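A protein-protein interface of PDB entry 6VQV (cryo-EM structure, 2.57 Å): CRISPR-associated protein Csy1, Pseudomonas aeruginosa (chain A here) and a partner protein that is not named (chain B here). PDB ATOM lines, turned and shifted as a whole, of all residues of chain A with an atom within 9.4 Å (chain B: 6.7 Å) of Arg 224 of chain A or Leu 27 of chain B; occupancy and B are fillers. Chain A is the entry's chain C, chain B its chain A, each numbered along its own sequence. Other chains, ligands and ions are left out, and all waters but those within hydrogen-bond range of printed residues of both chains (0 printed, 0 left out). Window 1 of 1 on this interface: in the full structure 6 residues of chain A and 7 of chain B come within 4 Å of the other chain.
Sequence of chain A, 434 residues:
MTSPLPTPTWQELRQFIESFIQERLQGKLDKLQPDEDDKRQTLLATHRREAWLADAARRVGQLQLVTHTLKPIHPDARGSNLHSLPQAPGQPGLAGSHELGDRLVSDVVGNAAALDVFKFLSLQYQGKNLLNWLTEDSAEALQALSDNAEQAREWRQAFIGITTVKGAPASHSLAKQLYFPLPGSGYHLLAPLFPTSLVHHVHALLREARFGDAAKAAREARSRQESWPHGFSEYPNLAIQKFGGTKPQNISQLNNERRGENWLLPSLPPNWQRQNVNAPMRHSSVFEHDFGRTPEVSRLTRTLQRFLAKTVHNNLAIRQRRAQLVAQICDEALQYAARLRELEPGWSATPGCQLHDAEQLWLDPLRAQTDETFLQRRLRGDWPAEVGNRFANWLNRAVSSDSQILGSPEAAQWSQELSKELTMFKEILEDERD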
ATOM      1  N   LYS A 216       7.050  17.289   9.263  1.00  0.00           N
ATOM      2  CA  LYS A 216       7.278  18.120   8.090  1.00  0.00           C
ATOM      3  C   LYS A 216       8.518  17.701   7.319  1.00  0.00           C
ATOM      4  O   LYS A 216       8.601  17.993   6.122  1.00  0.00           O
ATOM      5  CB  LYS A 216       7.375  19.596   8.479  1.00  0.00           C
ATOM      6  CG  LYS A 216       8.598  19.969   9.284  1.00  0.00           C
ATOM      7  CD  LYS A 216       8.582  21.448   9.625  1.00  0.00           C
ATOM      8  CE  LYS A 216       9.841  21.865  10.360  1.00  0.00           C
ATOM      9  NZ  LYS A 216       9.820  23.306  10.723  1.00  0.00           N
ATOM     10  N   ALA A 217       9.455  16.994   7.962  1.00  0.00           N
ATOM     11  CA  ALA A 217      10.541  16.354   7.225  1.00  0.00           C
ATOM     12  C   ALA A 217      10.003  15.325   6.238  1.00  0.00           C
ATOM     13  O   ALA A 217      10.420  15.291   5.076  1.00  0.00           O
ATOM     14  CB  ALA A 217      11.520  15.699   8.197  1.00  0.00           C
ATOM     15  N   ALA A 218       9.066  14.485   6.675  1.00  0.00           N
ATOM     16  CA  ALA A 218       8.478  13.504   5.778  1.00  0.00           C
ATOM     17  C   ALA A 218       7.497  14.129   4.802  1.00  0.00           C
ATOM     18  O   ALA A 218       7.284  13.577   3.722  1.00  0.00           O
ATOM     19  CB  ALA A 218       7.793  12.400   6.578  1.00  0.00           C
ATOM     20  N   ARG A 219       6.912  15.276   5.143  1.00  0.00           N
ATOM     21  CA  ARG A 219       6.147  16.023   4.148  1.00  0.00           C
ATOM     22  C   ARG A 219       7.054  16.585   3.058  1.00  0.00           C
ATOM     23  O   ARG A 219       6.637  16.690   1.901  1.00  0.00           O
ATOM     24  CB  ARG A 219       5.365  17.156   4.811  1.00  0.00           C
ATOM     25  CG  ARG A 219       4.236  16.719   5.720  1.00  0.00           C
ATOM     26  CD  ARG A 219       3.594  17.931   6.370  1.00  0.00           C
ATOM     27  NE  ARG A 219       2.588  17.577   7.365  1.00  0.00           N
ATOM     28  CZ  ARG A 219       1.292  17.446   7.103  1.00  0.00           C
ATOM     29  NH1 ARG A 219       0.838  17.644   5.873  1.00  0.00           N
ATOM     30  NH2 ARG A 219       0.447  17.124   8.071  1.00  0.00           N
ATOM     31  N   GLU A 220       8.286  16.960   3.411  1.00  0.00           N
ATOM     32  CA  GLU A 220       9.263  17.347   2.398  1.00  0.00           C
ATOM     33  C   GLU A 220       9.707  16.148   1.572  1.00  0.00           C
ATOM     34  O   GLU A 220       9.846  16.247   0.351  1.00  0.00           O
ATOM     35  CB  GLU A 220      10.475  18.002   3.055  1.00  0.00           C
ATOM     36  CG  GLU A 220      10.227  19.373   3.640  1.00  0.00           C
ATOM     37  CD  GLU A 220      11.428  19.897   4.398  1.00  0.00           C
ATOM     38  OE1 GLU A 220      12.398  19.129   4.575  1.00  0.00           O
ATOM     39  OE2 GLU A 220      11.404  21.071   4.822  1.00  0.00           O
ATOM     40  N   ALA A 221       9.943  15.009   2.222  1.00  0.00           N
ATOM     41  CA  ALA A 221      10.347  13.786   1.533  1.00  0.00           C
ATOM     42  C   ALA A 221       9.230  13.164   0.712  1.00  0.00           C
ATOM     43  O   ALA A 221       9.504  12.275  -0.097  1.00  0.00           O
ATOM     44  CB  ALA A 221      10.861  12.755   2.526  1.00  0.00           C
ATOM     45  N   ARG A 222       7.983  13.560   0.939  1.00  0.00           N
ATOM     46  CA  ARG A 222       6.902  13.107   0.079  1.00  0.00           C
ATOM     47  C   ARG A 222       6.966  13.803  -1.273  1.00  0.00           C
ATOM     48  O   ARG A 222       6.680  13.189  -2.306  1.00  0.00           O
ATOM     49  CB  ARG A 222       5.565  13.354   0.785  1.00  0.00           C
ATOM     50  CG  ARG A 222       4.311  12.784   0.132  1.00  0.00           C
ATOM     51  CD  ARG A 222       3.589  13.817  -0.709  1.00  0.00           C
ATOM     52  NE  ARG A 222       2.320  13.329  -1.226  1.00  0.00           N
ATOM     53  CZ  ARG A 222       1.152  13.549  -0.640  1.00  0.00           C
ATOM     54  NH1 ARG A 222       1.091  14.272   0.468  1.00  0.00           N
ATOM     55  NH2 ARG A 222       0.040  13.070  -1.175  1.00  0.00           N
ATOM     56  N   SER A 223       7.343  15.082  -1.282  1.00  0.00           N
ATOM     57  CA  SER A 223       7.394  15.844  -2.522  1.00  0.00           C
ATOM     58  C   SER A 223       8.593  15.449  -3.371  1.00  0.00           C
ATOM     59  O   SER A 223       8.488  15.366  -4.598  1.00  0.00           O
ATOM     60  CB  SER A 223       7.433  17.338  -2.213  1.00  0.00           C
ATOM     61  OG  SER A 223       8.644  17.679  -1.573  1.00  0.00           O
ATOM     62  N   ARG A 224       9.730  15.190  -2.736  1.00  0.00           N
ATOM     63  CA  ARG A 224      10.932  14.751  -3.428  1.00  0.00           C
ATOM     64  C   ARG A 224      10.952  13.251  -3.690  1.00  0.00           C
ATOM     65  O   ARG A 224      11.928  12.767  -4.265  1.00  0.00           O
ATOM     66  CB  ARG A 224      12.166  15.137  -2.618  1.00  0.00           C
ATOM     67  CG  ARG A 224      12.346  16.628  -2.442  1.00  0.00           C
ATOM     68  CD  ARG A 224      13.564  16.917  -1.588  1.00  0.00           C
ATOM     69  NE  ARG A 224      13.392  16.433  -0.224  1.00  0.00           N
ATOM     70  CZ  ARG A 224      14.343  16.459   0.701  1.00  0.00           C
ATOM     71  NH1 ARG A 224      15.538  16.947   0.406  1.00  0.00           N
ATOM     72  NH2 ARG A 224      14.098  15.998   1.918  1.00  0.00           N
ATOM     73  N   GLN A 225       9.919  12.527  -3.251  1.00  0.00           N
ATOM     74  CA  GLN A 225       9.750  11.084  -3.457  1.00  0.00           C
ATOM     75  C   GLN A 225      10.906  10.270  -2.875  1.00  0.00           C
ATOM     76  O   GLN A 225      11.299   9.240  -3.422  1.00  0.00           O
ATOM     77  CB  GLN A 225       9.536  10.752  -4.934  1.00  0.00           C
ATOM     78  CG  GLN A 225       8.252  11.298  -5.490  1.00  0.00           C
ATOM     79  CD  GLN A 225       8.063  10.953  -6.943  1.00  0.00           C
ATOM     80  OE1 GLN A 225       8.915  10.315  -7.552  1.00  0.00           O
ATOM     81  NE2 GLN A 225       6.948  11.384  -7.514  1.00  0.00           N
ATOM     82  N   GLU A 226      11.433  10.720  -1.738  1.00  0.00           N
ATOM     83  CA  GLU A 226      12.511  10.031  -1.039  1.00  0.00           C
ATOM     84  C   GLU A 226      11.930   8.892  -0.205  1.00  0.00           C
ATOM     85  O   GLU A 226      10.764   8.524  -0.353  1.00  0.00           O
ATOM     86  CB  GLU A 226      13.292  11.024  -0.190  1.00  0.00           C
ATOM     87  CG  GLU A 226      13.987  12.075  -1.008  1.00  0.00           C
ATOM     88  CD  GLU A 226      14.689  13.102  -0.160  1.00  0.00           C
ATOM     89  OE1 GLU A 226      14.506  13.094   1.073  1.00  0.00           O
ATOM     90  OE2 GLU A 226      15.438  13.916  -0.735  1.00  0.00           O
ATOM     91  N   SER A 227      12.727   8.315   0.689  1.00  0.00           N
ATOM     92  CA  SER A 227      12.232   7.219   1.518  1.00  0.00           C
ATOM     93  C   SER A 227      13.041   7.123   2.800  1.00  0.00           C
ATOM     94  O   SER A 227      14.262   6.948   2.753  1.00  0.00           O
ATOM     95  CB  SER A 227      12.280   5.892   0.762  1.00  0.00           C
ATOM     96  OG  SER A 227      11.738   4.849   1.549  1.00  0.00           O
ATOM     97  N   TRP A 228      12.360   7.257   3.934  1.00  0.00           N
ATOM     98  CA  TRP A 228      12.881   6.845   5.230  1.00  0.00           C
ATOM     99  C   TRP A 228      11.694   6.295   6.016  1.00  0.00           C
ATOM    100  O   TRP A 228      10.544   6.588   5.658  1.00  0.00           O
ATOM    101  CB  TRP A 228      13.581   8.003   5.981  1.00  0.00           C
ATOM    102  CG  TRP A 228      12.825   9.231   6.270  1.00  0.00           C
ATOM    103  CD1 TRP A 228      11.830   9.377   7.176  1.00  0.00           C
ATOM    104  CD2 TRP A 228      13.125  10.543   5.789  1.00  0.00           C
ATOM    105  NE1 TRP A 228      11.420  10.684   7.225  1.00  0.00           N
ATOM    106  CE2 TRP A 228      12.209  11.422   6.386  1.00  0.00           C
ATOM    107  CE3 TRP A 228      14.051  11.053   4.879  1.00  0.00           C
ATOM    108  CZ2 TRP A 228      12.195  12.778   6.109  1.00  0.00           C
ATOM    109  CZ3 TRP A 228      14.033  12.403   4.603  1.00  0.00           C
ATOM    110  CH2 TRP A 228      13.114  13.251   5.221  1.00  0.00           C
ATOM    111  N   TYR B   5      11.904   7.015 -14.352  1.00  0.00           N
ATOM    112  CA  TYR B   5      11.342   8.266 -14.839  1.00  0.00           C
ATOM    113  C   TYR B   5      11.551   8.342 -16.341  1.00  0.00           C
ATOM    114  O   TYR B   5      12.297   7.556 -16.924  1.00  0.00           O
ATOM    115  CB  TYR B   5      11.979   9.475 -14.151  1.00  0.00           C
ATOM    116  CG  TYR B   5      11.740   9.508 -12.668  1.00  0.00           C
ATOM    117  CD1 TYR B   5      10.557  10.007 -12.150  1.00  0.00           C
ATOM    118  CD2 TYR B   5      12.701   9.043 -11.784  1.00  0.00           C
ATOM    119  CE1 TYR B   5      10.337  10.045 -10.793  1.00  0.00           C
ATOM    120  CE2 TYR B   5      12.491   9.076 -10.429  1.00  0.00           C
ATOM    121  CZ  TYR B   5      11.306   9.578  -9.940  1.00  0.00           C
ATOM    122  OH  TYR B   5      11.093   9.613  -8.586  1.00  0.00           O
ATOM    123  N   ALA B  24      16.358   6.561 -11.159  1.00  0.00           N
ATOM    124  CA  ALA B  24      16.709   7.531 -10.134  1.00  0.00           C
ATOM    125  C   ALA B  24      16.010   7.187  -8.832  1.00  0.00           C
ATOM    126  O   ALA B  24      14.932   6.593  -8.813  1.00  0.00           O
ATOM    127  CB  ALA B  24      16.354   8.958 -10.551  1.00  0.00           C
ATOM    128  N   THR B  25      16.643   7.584  -7.733  1.00  0.00           N
ATOM    129  CA  THR B  25      16.092   7.316  -6.414  1.00  0.00           C
ATOM    130  C   THR B  25      14.988   8.304  -6.060  1.00  0.00           C
ATOM    131  O   THR B  25      13.873   7.903  -5.711  1.00  0.00           O
ATOM    132  CB  THR B  25      17.210   7.360  -5.376  1.00  0.00           C
ATOM    133  OG1 THR B  25      17.781   8.673  -5.356  1.00  0.00           O
ATOM    134  CG2 THR B  25      18.287   6.357  -5.737  1.00  0.00           C
ATOM    135  N   SER B  26      15.276   9.597  -6.155  1.00  0.00           N
ATOM    136  CA  SER B  26      14.334  10.635  -5.775  1.00  0.00           C
ATOM    137  C   SER B  26      14.003  11.482  -6.998  1.00  0.00           C
ATOM    138  O   SER B  26      14.557  11.293  -8.082  1.00  0.00           O
ATOM    139  CB  SER B  26      14.899  11.496  -4.639  1.00  0.00           C
ATOM    140  OG  SER B  26      16.026  12.241  -5.060  1.00  0.00           O
ATOM    141  N   LEU B  27      13.070  12.417  -6.821  1.00  0.00           N
ATOM    142  CA  LEU B  27      12.777  13.363  -7.890  1.00  0.00           C
ATOM    143  C   LEU B  27      13.862  14.425  -7.988  1.00  0.00           C
ATOM    144  O   LEU B  27      14.103  14.967  -9.071  1.00  0.00           O
ATOM    145  CB  LEU B  27      11.407  14.003  -7.665  1.00  0.00           C
ATOM    146  CG  LEU B  27      10.857  14.938  -8.739  1.00  0.00           C
ATOM    147  CD1 LEU B  27      10.698  14.191 -10.038  1.00  0.00           C
ATOM    148  CD2 LEU B  27       9.535  15.535  -8.309  1.00  0.00           C
ATOM    149  N   SER B  28      14.543  14.714  -6.879  1.00  0.00           N
ATOM    150  CA  SER B  28      15.658  15.651  -6.919  1.00  0.00           C
ATOM    151  C   SER B  28      16.855  15.062  -7.650  1.00  0.00           C
ATOM    152  O   SER B  28      17.588  15.792  -8.326  1.00  0.00           O
ATOM    153  CB  SER B  28      16.049  16.056  -5.502  1.00  0.00           C
ATOM    154  OG  SER B  28      14.976  16.708  -4.850  1.00  0.00           O
ATOM    155  N   GLN B  29      17.058  13.747  -7.542  1.00  0.00           N
ATOM    156  CA  GLN B  29      18.083  13.083  -8.339  1.00  0.00           C
ATOM    157  C   GLN B  29      17.746  13.136  -9.822  1.00  0.00           C
ATOM    158  O   GLN B  29      18.639  13.334 -10.657  1.00  0.00           O
ATOM    159  CB  GLN B  29      18.241  11.635  -7.875  1.00  0.00           C
ATOM    160  CG  GLN B  29      19.361  10.866  -8.551  1.00  0.00           C
ATOM    161  CD  GLN B  29      20.728  11.378  -8.164  1.00  0.00           C
ATOM    162  OE1 GLN B  29      20.975  11.691  -7.002  1.00  0.00           O
ATOM    163  NE2 GLN B  29      21.627  11.464  -9.136  1.00  0.00           N
ATOM    164  N   ALA B  30      16.463  12.995 -10.160  1.00  0.00           N
ATOM    165  CA  ALA B  30      16.035  13.130 -11.545  1.00  0.00           C
ATOM    166  C   ALA B  30      16.205  14.553 -12.048  1.00  0.00           C
ATOM    167  O   ALA B  30      16.575  14.751 -13.205  1.00  0.00           O
ATOM    168  CB  ALA B  30      14.584  12.689 -11.695  1.00  0.00           C
ATOM    169  N   LYS B  31      15.970  15.552 -11.197  1.00  0.00           N
ATOM    170  CA  LYS B  31      16.221  16.933 -11.594  1.00  0.00           C
ATOM    171  C   LYS B  31      17.702  17.227 -11.750  1.00  0.00           C
ATOM    172  O   LYS B  31      18.071  18.033 -12.608  1.00  0.00           O
ATOM    173  CB  LYS B  31      15.613  17.898 -10.584  1.00  0.00           C
ATOM    174  CG  LYS B  31      14.108  17.918 -10.572  1.00  0.00           C
ATOM    175  CD  LYS B  31      13.606  18.927  -9.570  1.00  0.00           C
ATOM    176  CE  LYS B  31      12.103  18.947  -9.518  1.00  0.00           C
ATOM    177  NZ  LYS B  31      11.632  19.930  -8.516  1.00  0.00           N
ATOM    178  N   ARG B  32      18.559  16.595 -10.948  1.00  0.00           N
ATOM    179  CA  ARG B  32      19.996  16.763 -11.129  1.00  0.00           C
ATOM    180  C   ARG B  32      20.488  16.123 -12.418  1.00  0.00           C
ATOM    181  O   ARG B  32      21.303  16.718 -13.130  1.00  0.00           O
ATOM    182  CB  ARG B  32      20.767  16.187  -9.944  1.00  0.00           C
ATOM    183  CG  ARG B  32      20.703  17.024  -8.691  1.00  0.00           C
ATOM    184  CD  ARG B  32      21.716  16.542  -7.666  1.00  0.00           C
ATOM    185  NE  ARG B  32      21.419  15.201  -7.180  1.00  0.00           N
ATOM    186  CZ  ARG B  32      20.621  14.950  -6.149  1.00  0.00           C
ATOM    187  NH1 ARG B  32      20.041  15.951  -5.503  1.00  0.00           N
ATOM    188  NH2 ARG B  32      20.400  13.703  -5.764  1.00  0.00           N
ATOM    189  N   ILE B  47      10.066  16.066 -16.757  1.00  0.00           N
ATOM    190  CA  ILE B  47      10.203  14.798 -16.057  1.00  0.00           C
ATOM    191  C   ILE B  47       8.824  14.181 -15.910  1.00  0.00           C
ATOM    192  O   ILE B  47       7.901  14.828 -15.404  1.00  0.00           O
ATOM    193  CB  ILE B  47      10.866  14.975 -14.687  1.00  0.00           C
ATOM    194  CG1 ILE B  47      12.223  15.638 -14.852  1.00  0.00           C
ATOM    195  CG2 ILE B  47      11.060  13.638 -14.038  1.00  0.00           C
ATOM    196  CD1 ILE B  47      12.840  16.035 -13.564  1.00  0.00           C
ATOM    197  N   LEU B  55       5.615  15.470 -13.941  1.00  0.00           N
ATOM    198  CA  LEU B  55       6.050  15.708 -12.574  1.00  0.00           C
ATOM    199  C   LEU B  55       6.651  17.090 -12.391  1.00  0.00           C
ATOM    200  O   LEU B  55       6.270  17.804 -11.457  1.00  0.00           O
ATOM    201  CB  LEU B  55       7.058  14.632 -12.154  1.00  0.00           C
ATOM    202  CG  LEU B  55       6.537  13.198 -12.190  1.00  0.00           C
ATOM    203  CD1 LEU B  55       7.639  12.233 -11.865  1.00  0.00           C
ATOM    204  CD2 LEU B  55       5.388  13.013 -11.242  1.00  0.00           C
ATOM    205  N   ALA B  56       7.571  17.495 -13.260  1.00  0.00           N
ATOM    206  CA  ALA B  56       8.206  18.801 -13.159  1.00  0.00           C
ATOM    207  C   ALA B  56       8.703  19.201 -14.535  1.00  0.00           C
ATOM    208  O   ALA B  56       8.843  18.362 -15.424  1.00  0.00           O
ATOM    209  CB  ALA B  56       9.361  18.787 -12.157  1.00  0.00           C
ATOM    210  N   ASP B  66       7.161  22.614 -10.519  1.00  0.00           N
ATOM    211  CA  ASP B  66       6.578  21.332 -10.169  1.00  0.00           C
ATOM    212  C   ASP B  66       5.121  21.268 -10.614  1.00  0.00           C
ATOM    213  O   ASP B  66       4.412  22.275 -10.666  1.00  0.00           O
ATOM    214  CB  ASP B  66       6.690  21.086  -8.670  1.00  0.00           C
ATOM    215  CG  ASP B  66       8.110  20.817  -8.235  1.00  0.00           C
ATOM    216  OD1 ASP B  66       8.871  20.228  -9.028  1.00  0.00           O
ATOM    217  OD2 ASP B  66       8.477  21.208  -7.110  1.00  0.00           O
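The side-chain hydroxyl (OH) of Tyr 5 of chain B is in hydrogen-bond range of the side-chain amide oxygen (OE1) of Gln 225 of chain A (2.5 Å).
The backbone NH of Leu 27 of chain B is in hydrogen-bond range of the backbone carbonyl oxygen of Arg 224 of chain A.
The side-chain hydroxyl (OG) of Ser 26 of chain B sits close to the backbone NH (N) of Ser 28 of chain B (3.4 Å).
The side-chain hydroxyl of Ser 26 of chain B lies within hydrogen-bond range of the backbone NH of Gln 29 of chain B (3.1 Å).
OG of Ser 223 of chain A sits at hydrogen-bond distance from O of Glu 220 of chain A, 2.7 Å away.
O of Ala 221 of chain A sits at hydrogen-bond distance from N of Glu 226 of chain A.
The side-chain carboxylate (OE1) of Glu 226 of chain A lies within salt-bridge range of the guanidinium group (NH2) of Arg 224 of chain A, 3.1 Å away.
Among the printed residues, merely in contact across the chains: Ser 223 of chain A with Leu 27 of chain B, Arg 224 of chain A with Ser 26 of chain B, Arg 224 of chain A with Ser 28 of chain B, Gln 225 of chain A with Thr 25 of chain B and Glu 226 of chain A with Ser 26 of chain B.
Leu 27 of chain B touches just these residues of chain A: Ser 223 and Arg 224.
Ser 26 of chain B touches two residues of chain A.
Ser 28 of chain B touches one residue of chain A.
Ala 30 of chain B touches none of the printed residues of chain A.
Printed residues of chain B within 4 Å of Glu 226 of chain A: Ser 26 (3.8 Å).
Of the printed residues of chain B, Gln 225 of chain A touches Tyr 5 (2.5 Å) and Thr 25 (3.7 Å).
Printed residues of chain B within 4 Å of Ser 223 of chain A: Leu 27 (3.9 Å).
Ile 47 of chain B touches none of the printed residues of chain A.
Ala 218 of chain A touches none of the printed residues of chain B.
The nearest printed residue of chain B that does not touch Ser 223 of chain A is Asp 66 of chain B (6.3 Å).
Hydrophobic or aromatic side chains of chain B that line the printed part of chain A: Tyr 5 and Leu 27.
Among the printed residues, 7 pairs touch across the chains.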
